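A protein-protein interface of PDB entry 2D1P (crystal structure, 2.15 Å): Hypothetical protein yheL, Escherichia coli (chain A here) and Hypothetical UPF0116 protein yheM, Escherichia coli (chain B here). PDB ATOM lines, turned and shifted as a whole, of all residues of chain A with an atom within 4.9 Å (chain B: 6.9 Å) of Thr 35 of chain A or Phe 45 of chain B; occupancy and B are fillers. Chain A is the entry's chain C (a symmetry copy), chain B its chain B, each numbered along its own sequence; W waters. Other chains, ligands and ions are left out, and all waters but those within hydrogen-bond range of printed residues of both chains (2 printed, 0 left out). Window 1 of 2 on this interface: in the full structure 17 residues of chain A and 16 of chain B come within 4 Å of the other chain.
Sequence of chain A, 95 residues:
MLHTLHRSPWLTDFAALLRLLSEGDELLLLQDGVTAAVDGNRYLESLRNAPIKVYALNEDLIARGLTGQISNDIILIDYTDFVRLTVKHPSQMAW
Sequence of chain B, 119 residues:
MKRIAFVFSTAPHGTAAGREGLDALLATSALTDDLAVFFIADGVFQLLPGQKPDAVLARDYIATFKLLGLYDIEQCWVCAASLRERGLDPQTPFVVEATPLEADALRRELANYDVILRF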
ATOM      1  N   SER A   8     -17.178 -21.157 -24.396  1.00  0.00           N
ATOM      2  CA  SER A   8     -17.353 -22.594 -24.511  1.00  0.00           C
ATOM      3  C   SER A   8     -18.105 -22.876 -25.807  1.00  0.00           C
ATOM      4  O   SER A   8     -19.090 -22.205 -26.111  1.00  0.00           O
ATOM      5  CB  SER A   8     -18.166 -23.105 -23.327  1.00  0.00           C
ATOM      6  OG  SER A   8     -18.687 -24.389 -23.594  1.00  0.00           O
ATOM      7  N   PRO A   9     -17.649 -23.867 -26.589  1.00  0.00           N
ATOM      8  CA  PRO A   9     -18.335 -24.186 -27.844  1.00  0.00           C
ATOM      9  C   PRO A   9     -19.810 -24.509 -27.629  1.00  0.00           C
ATOM     10  O   PRO A   9     -20.638 -24.277 -28.517  1.00  0.00           O
ATOM     11  CB  PRO A   9     -17.536 -25.370 -28.392  1.00  0.00           C
ATOM     12  CG  PRO A   9     -16.895 -25.963 -27.168  1.00  0.00           C
ATOM     13  CD  PRO A   9     -16.496 -24.755 -26.379  1.00  0.00           C
ATOM     14  N   TRP A  10     -20.135 -25.024 -26.442  1.00  0.00           N
ATOM     15  CA  TRP A  10     -21.513 -25.367 -26.089  1.00  0.00           C
ATOM     16  C   TRP A  10     -22.395 -24.124 -25.934  1.00  0.00           C
ATOM     17  O   TRP A  10     -23.623 -24.218 -26.005  1.00  0.00           O
ATOM     18  CB  TRP A  10     -21.541 -26.176 -24.777  1.00  0.00           C
ATOM     19  CG  TRP A  10     -21.136 -27.611 -24.940  1.00  0.00           C
ATOM     20  CD1 TRP A  10     -21.958 -28.670 -25.225  1.00  0.00           C
ATOM     21  CD2 TRP A  10     -19.805 -28.132 -24.923  1.00  0.00           C
ATOM     22  NE1 TRP A  10     -21.218 -29.812 -25.392  1.00  0.00           N
ATOM     23  CE2 TRP A  10     -19.892 -29.512 -25.213  1.00  0.00           C
ATOM     24  CE3 TRP A  10     -18.543 -27.566 -24.693  1.00  0.00           C
ATOM     25  CZ2 TRP A  10     -18.763 -30.336 -25.285  1.00  0.00           C
ATOM     26  CZ3 TRP A  10     -17.416 -28.387 -24.763  1.00  0.00           C
ATOM     27  CH2 TRP A  10     -17.535 -29.758 -25.059  1.00  0.00           C
ATOM     28  N   ASP A  32     -12.379 -19.880 -22.071  1.00  0.00           N
ATOM     29  CA  ASP A  32     -13.234 -21.067 -22.055  1.00  0.00           C
ATOM     30  C   ASP A  32     -13.283 -21.814 -23.387  1.00  0.00           C
ATOM     31  O   ASP A  32     -13.820 -22.930 -23.461  1.00  0.00           O
ATOM     32  CB  ASP A  32     -14.661 -20.708 -21.631  1.00  0.00           C
ATOM     33  CG  ASP A  32     -14.768 -20.376 -20.150  1.00  0.00           C
ATOM     34  OD1 ASP A  32     -13.848 -20.741 -19.381  1.00  0.00           O
ATOM     35  OD2 ASP A  32     -15.780 -19.758 -19.752  1.00  0.00           O
ATOM     36  N   GLY A  33     -12.735 -21.202 -24.434  1.00  0.00           N
ATOM     37  CA  GLY A  33     -12.734 -21.847 -25.733  1.00  0.00           C
ATOM     38  C   GLY A  33     -11.837 -23.080 -25.799  1.00  0.00           C
ATOM     39  O   GLY A  33     -12.064 -23.974 -26.599  1.00  0.00           O
ATOM     40  N   VAL A  34     -10.820 -23.143 -24.951  1.00  0.00           N
ATOM     41  CA  VAL A  34      -9.903 -24.271 -24.988  1.00  0.00           C
ATOM     42  C   VAL A  34     -10.550 -25.621 -24.698  1.00  0.00           C
ATOM     43  O   VAL A  34      -9.924 -26.651 -24.895  1.00  0.00           O
ATOM     44  CB  VAL A  34      -8.716 -24.060 -24.030  1.00  0.00           C
ATOM     45  CG1 VAL A  34      -7.962 -22.798 -24.421  1.00  0.00           C
ATOM     46  CG2 VAL A  34      -9.206 -23.975 -22.599  1.00  0.00           C
ATOM     47  N   THR A  35     -11.794 -25.622 -24.232  1.00  0.00           N
ATOM     48  CA  THR A  35     -12.473 -26.884 -23.963  1.00  0.00           C
ATOM     49  C   THR A  35     -12.772 -27.625 -25.269  1.00  0.00           C
ATOM     50  O   THR A  35     -12.945 -28.842 -25.270  1.00  0.00           O
ATOM     51  CB  THR A  35     -13.793 -26.677 -23.205  1.00  0.00           C
ATOM     52  OG1 THR A  35     -14.579 -25.675 -23.866  1.00  0.00           O
ATOM     53  CG2 THR A  35     -13.515 -26.270 -21.760  1.00  0.00           C
ATOM     54  N   ALA A  36     -12.822 -26.894 -26.378  1.00  0.00           N
ATOM     55  CA  ALA A  36     -13.096 -27.517 -27.671  1.00  0.00           C
ATOM     56  C   ALA A  36     -11.876 -28.296 -28.166  1.00  0.00           C
ATOM     57  O   ALA A  36     -11.942 -28.989 -29.181  1.00  0.00           O
ATOM     58  CB  ALA A  36     -13.490 -26.457 -28.696  1.00  0.00           C
ATOM     59  N   ALA A  37     -10.768 -28.187 -27.442  1.00  0.00           N
ATOM     60  CA  ALA A  37      -9.542 -28.875 -27.822  1.00  0.00           C
ATOM     61  C   ALA A  37      -9.349 -30.200 -27.085  1.00  0.00           C
ATOM     62  O   ALA A  37      -8.368 -30.905 -27.317  1.00  0.00           O
ATOM     63  CB  ALA A  37      -8.343 -27.976 -27.570  1.00  0.00           C
ATOM     64  N   VAL A  38     -10.283 -30.537 -26.203  1.00  0.00           N
ATOM     65  CA  VAL A  38     -10.175 -31.772 -25.443  1.00  0.00           C
ATOM     66  C   VAL A  38     -10.462 -32.996 -26.311  1.00  0.00           C
ATOM     67  O   VAL A  38     -11.494 -33.084 -26.976  1.00  0.00           O
ATOM     68  CB  VAL A  38     -11.119 -31.762 -24.223  1.00  0.00           C
ATOM     69  CG1 VAL A  38     -11.035 -33.094 -23.473  1.00  0.00           C
ATOM     70  CG2 VAL A  38     -10.731 -30.625 -23.297  1.00  0.00           C
ATOM     71  N   ASN A  41     -14.091 -34.638 -27.379  1.00  0.00           N
ATOM     72  CA  ASN A  41     -15.297 -33.832 -27.178  1.00  0.00           C
ATOM     73  C   ASN A  41     -16.049 -33.771 -28.503  1.00  0.00           C
ATOM     74  O   ASN A  41     -15.443 -33.879 -29.564  1.00  0.00           O
ATOM     75  CB  ASN A  41     -14.959 -32.420 -26.674  1.00  0.00           C
ATOM     76  CG  ASN A  41     -14.538 -31.481 -27.785  1.00  0.00           C
ATOM     77  OD1 ASN A  41     -13.357 -31.345 -28.088  1.00  0.00           O
ATOM     78  ND2 ASN A  41     -15.515 -30.835 -28.403  1.00  0.00           N
ATOM     79  N   LEU A  66      -6.162 -28.950 -18.234  1.00  0.00           N
ATOM     80  CA  LEU A  66      -6.435 -29.748 -19.421  1.00  0.00           C
ATOM     81  C   LEU A  66      -5.220 -30.006 -20.306  1.00  0.00           C
ATOM     82  O   LEU A  66      -5.353 -30.588 -21.379  1.00  0.00           O
ATOM     83  CB  LEU A  66      -7.522 -29.060 -20.245  1.00  0.00           C
ATOM     84  CG  LEU A  66      -8.898 -28.961 -19.587  1.00  0.00           C
ATOM     85  CD1 LEU A  66      -9.779 -28.011 -20.382  1.00  0.00           C
ATOM     86  CD2 LEU A  66      -9.529 -30.351 -19.517  1.00  0.00           C
ATOM     87  N   THR B  10     -21.417 -24.013 -15.473  1.00  0.00           N
ATOM     88  CA  THR B  10     -20.476 -23.268 -16.294  1.00  0.00           C
ATOM     89  C   THR B  10     -19.040 -23.674 -16.035  1.00  0.00           C
ATOM     90  O   THR B  10     -18.709 -24.152 -14.953  1.00  0.00           O
ATOM     91  CB  THR B  10     -20.608 -21.762 -16.048  1.00  0.00           C
ATOM     92  OG1 THR B  10     -20.107 -21.441 -14.744  1.00  0.00           O
ATOM     93  CG2 THR B  10     -22.065 -21.349 -16.129  1.00  0.00           C
ATOM     94  N   ALA B  11     -18.190 -23.483 -17.038  1.00  0.00           N
ATOM     95  CA  ALA B  11     -16.780 -23.815 -16.922  1.00  0.00           C
ATOM     96  C   ALA B  11     -16.093 -22.804 -16.007  1.00  0.00           C
ATOM     97  O   ALA B  11     -16.532 -21.662 -15.886  1.00  0.00           O
ATOM     98  CB  ALA B  11     -16.139 -23.813 -18.295  1.00  0.00           C
ATOM     99  N   PRO B  12     -15.002 -23.212 -15.347  1.00  0.00           N
ATOM    100  CA  PRO B  12     -14.280 -22.314 -14.440  1.00  0.00           C
ATOM    101  C   PRO B  12     -13.390 -21.264 -15.101  1.00  0.00           C
ATOM    102  O   PRO B  12     -12.928 -21.440 -16.234  1.00  0.00           O
ATOM    103  CB  PRO B  12     -13.456 -23.277 -13.604  1.00  0.00           C
ATOM    104  CG  PRO B  12     -13.096 -24.331 -14.615  1.00  0.00           C
ATOM    105  CD  PRO B  12     -14.429 -24.568 -15.305  1.00  0.00           C
ATOM    106  N   HIS B  13     -13.167 -20.173 -14.367  1.00  0.00           N
ATOM    107  CA  HIS B  13     -12.290 -19.082 -14.776  1.00  0.00           C
ATOM    108  C   HIS B  13     -12.765 -18.132 -15.889  1.00  0.00           C
ATOM    109  O   HIS B  13     -12.604 -16.913 -15.769  1.00  0.00           O
ATOM    110  CB  HIS B  13     -10.921 -19.684 -15.102  1.00  0.00           C
ATOM    111  CG  HIS B  13     -10.543 -20.808 -14.184  1.00  0.00           C
ATOM    112  ND1 HIS B  13     -10.579 -20.689 -12.811  1.00  0.00           N
ATOM    113  CD2 HIS B  13     -10.173 -22.086 -14.441  1.00  0.00           C
ATOM    114  CE1 HIS B  13     -10.251 -21.844 -12.262  1.00  0.00           C
ATOM    115  NE2 HIS B  13      -9.999 -22.708 -13.229  1.00  0.00           N
ATOM    116  N   PHE B  39     -23.285 -31.086 -10.708  1.00  0.00           N
ATOM    117  CA  PHE B  39     -22.346 -30.572 -11.691  1.00  0.00           C
ATOM    118  C   PHE B  39     -22.817 -31.087 -13.050  1.00  0.00           C
ATOM    119  O   PHE B  39     -22.708 -32.282 -13.350  1.00  0.00           O
ATOM    120  CB  PHE B  39     -20.933 -31.061 -11.369  1.00  0.00           C
ATOM    121  CG  PHE B  39     -20.358 -30.457 -10.110  1.00  0.00           C
ATOM    122  CD1 PHE B  39     -19.666 -29.243 -10.154  1.00  0.00           C
ATOM    123  CD2 PHE B  39     -20.529 -31.088  -8.876  1.00  0.00           C
ATOM    124  CE1 PHE B  39     -19.148 -28.662  -8.978  1.00  0.00           C
ATOM    125  CE2 PHE B  39     -20.019 -30.522  -7.699  1.00  0.00           C
ATOM    126  CZ  PHE B  39     -19.325 -29.304  -7.748  1.00  0.00           C
ATOM    127  N   ILE B  40     -23.365 -30.177 -13.853  1.00  0.00           N
ATOM    128  CA  ILE B  40     -23.895 -30.513 -15.173  1.00  0.00           C
ATOM    129  C   ILE B  40     -23.349 -29.602 -16.267  1.00  0.00           C
ATOM    130  O   ILE B  40     -22.791 -28.537 -15.989  1.00  0.00           O
ATOM    131  CB  ILE B  40     -25.430 -30.401 -15.186  1.00  0.00           C
ATOM    132  CG1 ILE B  40     -25.845 -28.926 -15.164  1.00  0.00           C
ATOM    133  CG2 ILE B  40     -26.004 -31.113 -13.976  1.00  0.00           C
ATOM    134  CD1 ILE B  40     -27.340 -28.690 -15.271  1.00  0.00           C
ATOM    135  N   ALA B  41     -23.533 -30.018 -17.518  1.00  0.00           N
ATOM    136  CA  ALA B  41     -23.055 -29.251 -18.662  1.00  0.00           C
ATOM    137  C   ALA B  41     -21.582 -28.899 -18.444  1.00  0.00           C
ATOM    138  O   ALA B  41     -20.803 -29.750 -17.995  1.00  0.00           O
ATOM    139  CB  ALA B  41     -23.896 -27.988 -18.831  1.00  0.00           C
ATOM    140  N   ASP B  42     -21.203 -27.654 -18.745  1.00  0.00           N
ATOM    141  CA  ASP B  42     -19.816 -27.223 -18.567  1.00  0.00           C
ATOM    142  C   ASP B  42     -19.361 -27.217 -17.111  1.00  0.00           C
ATOM    143  O   ASP B  42     -18.162 -27.180 -16.835  1.00  0.00           O
ATOM    144  CB  ASP B  42     -19.593 -25.824 -19.154  1.00  0.00           C
ATOM    145  CG  ASP B  42     -19.465 -25.837 -20.666  1.00  0.00           C
ATOM    146  OD1 ASP B  42     -18.931 -26.824 -21.225  1.00  0.00           O
ATOM    147  OD2 ASP B  42     -19.882 -24.847 -21.297  1.00  0.00           O
ATOM    148  N   GLY B  43     -20.315 -27.241 -16.186  1.00  0.00           N
ATOM    149  CA  GLY B  43     -19.966 -27.244 -14.777  1.00  0.00           C
ATOM    150  C   GLY B  43     -19.101 -28.428 -14.366  1.00  0.00           C
ATOM    151  O   GLY B  43     -18.450 -28.378 -13.318  1.00  0.00           O
ATOM    152  N   VAL B  44     -19.081 -29.491 -15.171  1.00  0.00           N
ATOM    153  CA  VAL B  44     -18.264 -30.656 -14.835  1.00  0.00           C
ATOM    154  C   VAL B  44     -16.780 -30.279 -14.834  1.00  0.00           C
ATOM    155  O   VAL B  44     -15.967 -30.910 -14.145  1.00  0.00           O
ATOM    156  CB  VAL B  44     -18.492 -31.845 -15.826  1.00  0.00           C
ATOM    157  CG1 VAL B  44     -19.937 -32.315 -15.752  1.00  0.00           C
ATOM    158  CG2 VAL B  44     -18.131 -31.432 -17.252  1.00  0.00           C
ATOM    159  N   PHE B  45     -16.431 -29.247 -15.607  1.00  0.00           N
ATOM    160  CA  PHE B  45     -15.046 -28.786 -15.677  1.00  0.00           C
ATOM    161  C   PHE B  45     -14.580 -28.214 -14.323  1.00  0.00           C
ATOM    162  O   PHE B  45     -13.378 -28.099 -14.061  1.00  0.00           O
ATOM    163  CB  PHE B  45     -14.882 -27.720 -16.775  1.00  0.00           C
ATOM    164  CG  PHE B  45     -14.834 -28.275 -18.184  1.00  0.00           C
ATOM    165  CD1 PHE B  45     -13.781 -29.092 -18.598  1.00  0.00           C
ATOM    166  CD2 PHE B  45     -15.826 -27.951 -19.106  1.00  0.00           C
ATOM    167  CE1 PHE B  45     -13.716 -29.577 -19.910  1.00  0.00           C
ATOM    168  CE2 PHE B  45     -15.773 -28.430 -20.423  1.00  0.00           C
ATOM    169  CZ  PHE B  45     -14.714 -29.245 -20.822  1.00  0.00           C
ATOM    170  N   GLN B  46     -15.530 -27.852 -13.467  1.00  0.00           N
ATOM    171  CA  GLN B  46     -15.199 -27.308 -12.147  1.00  0.00           C
ATOM    172  C   GLN B  46     -14.448 -28.344 -11.319  1.00  0.00           C
ATOM    173  O   GLN B  46     -13.621 -27.996 -10.471  1.00  0.00           O
ATOM    174  CB  GLN B  46     -16.477 -26.933 -11.385  1.00  0.00           C
ATOM    175  CG  GLN B  46     -17.356 -25.919 -12.072  1.00  0.00           C
ATOM    176  CD  GLN B  46     -16.858 -24.491 -11.917  1.00  0.00           C
ATOM    177  OE1 GLN B  46     -17.242 -23.611 -12.688  1.00  0.00           O
ATOM    178  NE2 GLN B  46     -16.016 -24.254 -10.915  1.00  0.00           N
ATOM    179  N   LEU B  47     -14.750 -29.615 -11.584  1.00  0.00           N
ATOM    180  CA  LEU B  47     -14.191 -30.756 -10.857  1.00  0.00           C
ATOM    181  C   LEU B  47     -12.769 -31.220 -11.173  1.00  0.00           C
ATOM    182  O   LEU B  47     -12.193 -31.997 -10.416  1.00  0.00           O
ATOM    183  CB  LEU B  47     -15.130 -31.952 -11.032  1.00  0.00           C
ATOM    184  CG  LEU B  47     -16.587 -31.754 -10.624  1.00  0.00           C
ATOM    185  CD1 LEU B  47     -17.400 -32.943 -11.118  1.00  0.00           C
ATOM    186  CD2 LEU B  47     -16.696 -31.595  -9.113  1.00  0.00           C
ATOM    187  N   LEU B  48     -12.200 -30.764 -12.279  1.00  0.00           N
ATOM    188  CA  LEU B  48     -10.858 -31.202 -12.652  1.00  0.00           C
ATOM    189  C   LEU B  48      -9.738 -30.832 -11.685  1.00  0.00           C
ATOM    190  O   LEU B  48      -9.662 -29.706 -11.189  1.00  0.00           O
ATOM    191  CB  LEU B  48     -10.520 -30.698 -14.057  1.00  0.00           C
ATOM    192  CG  LEU B  48     -10.972 -31.579 -15.223  1.00  0.00           C
ATOM    193  CD1 LEU B  48     -12.392 -32.051 -15.032  1.00  0.00           C
ATOM    194  CD2 LEU B  48     -10.818 -30.803 -16.511  1.00  0.00           C
ATOM    195  N   PRO B  49      -8.849 -31.797 -11.395  1.00  0.00           N
ATOM    196  CA  PRO B  49      -7.725 -31.570 -10.482  1.00  0.00           C
ATOM    197  C   PRO B  49      -6.542 -30.938 -11.210  1.00  0.00           C
ATOM    198  O   PRO B  49      -6.483 -30.944 -12.436  1.00  0.00           O
ATOM    199  CB  PRO B  49      -7.414 -32.977  -9.976  1.00  0.00           C
ATOM    200  CG  PRO B  49      -7.647 -33.803 -11.203  1.00  0.00           C
ATOM    201  CD  PRO B  49      -8.958 -33.230 -11.742  1.00  0.00           C
ATOM    202  N   GLN B  51      -5.790 -27.805 -11.577  1.00  0.00           N
ATOM    203  CA  GLN B  51      -6.032 -26.507 -12.203  1.00  0.00           C
ATOM    204  C   GLN B  51      -5.130 -25.438 -11.579  1.00  0.00           C
ATOM    205  O   GLN B  51      -4.948 -25.395 -10.361  1.00  0.00           O
ATOM    206  CB  GLN B  51      -7.495 -26.101 -12.027  1.00  0.00           C
ATOM    207  CG  GLN B  51      -8.489 -27.036 -12.683  1.00  0.00           C
ATOM    208  CD  GLN B  51      -9.907 -26.531 -12.552  1.00  0.00           C
ATOM    209  OE1 GLN B  51     -10.218 -25.415 -12.968  1.00  0.00           O
ATOM    210  NE2 GLN B  51     -10.776 -27.344 -11.970  1.00  0.00           N
ATOM    211  N   ILE B  62     -10.767 -23.297  -6.775  1.00  0.00           N
ATOM    212  CA  ILE B  62     -11.013 -24.736  -6.894  1.00  0.00           C
ATOM    213  C   ILE B  62     -10.586 -25.418  -5.591  1.00  0.00           C
ATOM    214  O   ILE B  62     -11.245 -26.337  -5.108  1.00  0.00           O
ATOM    215  CB  ILE B  62     -10.212 -25.366  -8.075  1.00  0.00           C
ATOM    216  CG1 ILE B  62     -10.484 -24.599  -9.379  1.00  0.00           C
ATOM    217  CG2 ILE B  62     -10.624 -26.822  -8.266  1.00  0.00           C
ATOM    218  CD1 ILE B  62     -11.952 -24.597  -9.811  1.00  0.00           C
ATOM    219  N   SER B  82     -22.786 -35.461 -19.589  1.00  0.00           N
ATOM    220  CA  SER B  82     -21.983 -34.276 -19.872  1.00  0.00           C
ATOM    221  C   SER B  82     -20.494 -34.603 -19.999  1.00  0.00           C
ATOM    222  O   SER B  82     -19.825 -34.132 -20.922  1.00  0.00           O
ATOM    223  CB  SER B  82     -22.183 -33.213 -18.785  1.00  0.00           C
ATOM    224  OG  SER B  82     -21.239 -32.163 -18.950  1.00  0.00           O
ATOM    225  N   LEU B  83     -19.973 -35.399 -19.070  1.00  0.00           N
ATOM    226  CA  LEU B  83     -18.559 -35.775 -19.110  1.00  0.00           C
ATOM    227  C   LEU B  83     -18.222 -36.459 -20.435  1.00  0.00           C
ATOM    228  O   LEU B  83     -17.145 -36.241 -20.994  1.00  0.00           O
ATOM    229  CB  LEU B  83     -18.217 -36.712 -17.946  1.00  0.00           C
ATOM    230  CG  LEU B  83     -18.255 -36.136 -16.522  1.00  0.00           C
ATOM    231  CD1 LEU B  83     -18.246 -37.284 -15.508  1.00  0.00           C
ATOM    232  CD2 LEU B  83     -17.064 -35.221 -16.295  1.00  0.00           C
ATOM    233  N   ARG B  86     -17.932 -34.058 -23.361  1.00  0.00           N
ATOM    234  CA  ARG B  86     -16.715 -33.275 -23.246  1.00  0.00           C
ATOM    235  C   ARG B  86     -15.415 -34.061 -23.322  1.00  0.00           C
ATOM    236  O   ARG B  86     -14.330 -33.499 -23.165  1.00  0.00           O
ATOM    237  CB  ARG B  86     -16.798 -32.437 -21.966  1.00  0.00           C
ATOM    238  CG  ARG B  86     -17.859 -31.342 -22.104  1.00  0.00           C
ATOM    239  CD  ARG B  86     -18.387 -30.800 -20.789  1.00  0.00           C
ATOM    240  NE  ARG B  86     -19.304 -29.686 -21.037  1.00  0.00           N
ATOM    241  CZ  ARG B  86     -20.532 -29.808 -21.530  1.00  0.00           C
ATOM    242  NH1 ARG B  86     -21.029 -31.008 -21.825  1.00  0.00           N
ATOM    243  NH2 ARG B  86     -21.254 -28.721 -21.776  1.00  0.00           N
ATOM    244  N   GLY B  87     -15.528 -35.360 -23.591  1.00  0.00           N
ATOM    245  CA  GLY B  87     -14.353 -36.209 -23.708  1.00  0.00           C
ATOM    246  C   GLY B  87     -13.553 -36.359 -22.428  1.00  0.00           C
ATOM    247  O   GLY B  87     -12.334 -36.556 -22.460  1.00  0.00           O
ATOM    248  N   LEU B  88     -14.240 -36.280 -21.297  1.00  0.00           N
ATOM    249  CA  LEU B  88     -13.582 -36.394 -20.003  1.00  0.00           C
ATOM    250  C   LEU B  88     -13.676 -37.798 -19.390  1.00  0.00           C
ATOM    251  O   LEU B  88     -14.749 -38.398 -19.320  1.00  0.00           O
ATOM    252  CB  LEU B  88     -14.167 -35.351 -19.037  1.00  0.00           C
ATOM    253  CG  LEU B  88     -13.885 -33.883 -19.416  1.00  0.00           C
ATOM    254  CD1 LEU B  88     -14.763 -32.956 -18.597  1.00  0.00           C
ATOM    255  CD2 LEU B  88     -12.401 -33.558 -19.198  1.00  0.00           C
HETATM  256  O   HOH W   1     -17.312 -19.843 -17.511  1.00  0.00           O
HETATM  257  O   HOH W   2     -14.693 -30.583 -23.964  1.00  0.00           O
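O of Ala 41 of chain B sits at hydrogen-bond distance from NE of Arg 86 of chain B, 3.4 Å away. The side-chain carboxylate of Asp 42 of chain B lies within salt-bridge range of the guanidinium group of Arg 86 of chain B, 2.9 Å away. O of Leu 48 of chain B sits at hydrogen-bond distance from NE2 of Gln 51 of chain B. The guanidinium group (NH1) of Arg 86 of chain B sits at hydrogen-bond distance from the side-chain hydroxyl (OG) of Ser 82 of chain B (3.1 Å). The side-chain hydroxyl of Thr 35 of chain A sits at hydrogen-bond distance from the backbone carbonyl oxygen of Asp 32 of chain A (2.9 Å). The backbone carbonyl oxygen (O) of Ala 36 of chain A lies close to the side-chain amide oxygen (OD1) of Asn 41 of chain A (3.0 Å).
Hydrophobic or aromatic side chains of chain A within 4 Å of the printed part of chain B: Trp 10, Val 38 and Leu 66. Hydrophobic or aromatic side chains of chain B within 4 Å of the printed part of chain A: Ala 11, Phe 45 and Leu 48. Along chain B the printed residues that touch a printed residue of chain A span positions 11 to 87. Among the printed residues, 11 pairs touch across the chains. Among the printed residues, no Asp or Glu carboxylate lies within 4 Å of a Lys or Arg side-chain nitrogen of the other chain.
OD1 of Asp 42 of chain B touches CE3 of Trp 10 of chain A, at 3.6 Å. CG of Trp 10 of chain A touches NH2 of Arg 86 of chain B, 3.4 Å away. Ala 11 of chain B touches Asp 32 of chain A (CB to OD1, 3.98 Å). Thr 35 of chain A touches Phe 45 of chain B. Val 38 of chain A touches Arg 86 of chain B (CG1 to O, 3.3 Å). Val 38 of chain A touches Gly 87 of chain B. O of Arg 86 of chain B touches CB of Asn 41 of chain A, 3.7 Å away. Gly 87 of chain B touches Asn 41 of chain A. Leu 48 of chain B touches Leu 66 of chain A.
Printed residues of chain B within 4 Å of Trp 10 of chain A: Asp 42 (3.6 Å) and Arg 86 (3.4 Å). Thr 35 of chain A touches just one residue of chain B: Phe 45 (3.3 Å). Phe 45 of chain B touches just one residue of chain A: Thr 35. Printed residues of chain A within 4 Å of Leu 48 of chain B: Leu 66 (3.3 Å).
Water W1 lies within hydrogen-bond range of the backbone carbonyl oxygen (O) of Ala 11 of chain B and the side-chain carboxylate (OD2) of Asp 32 of chain A. Water W2 lies within hydrogen-bond range of O of Thr 35 of chain A and O of Arg 86 of chain B.
OD2 of Asp 42 of chain B is in hydrogen-bond range of OG of Ser 8 of chain A. OD1 of Asp 32 of chain A sits close to O of Pro 12 of chain B (3.4 Å).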
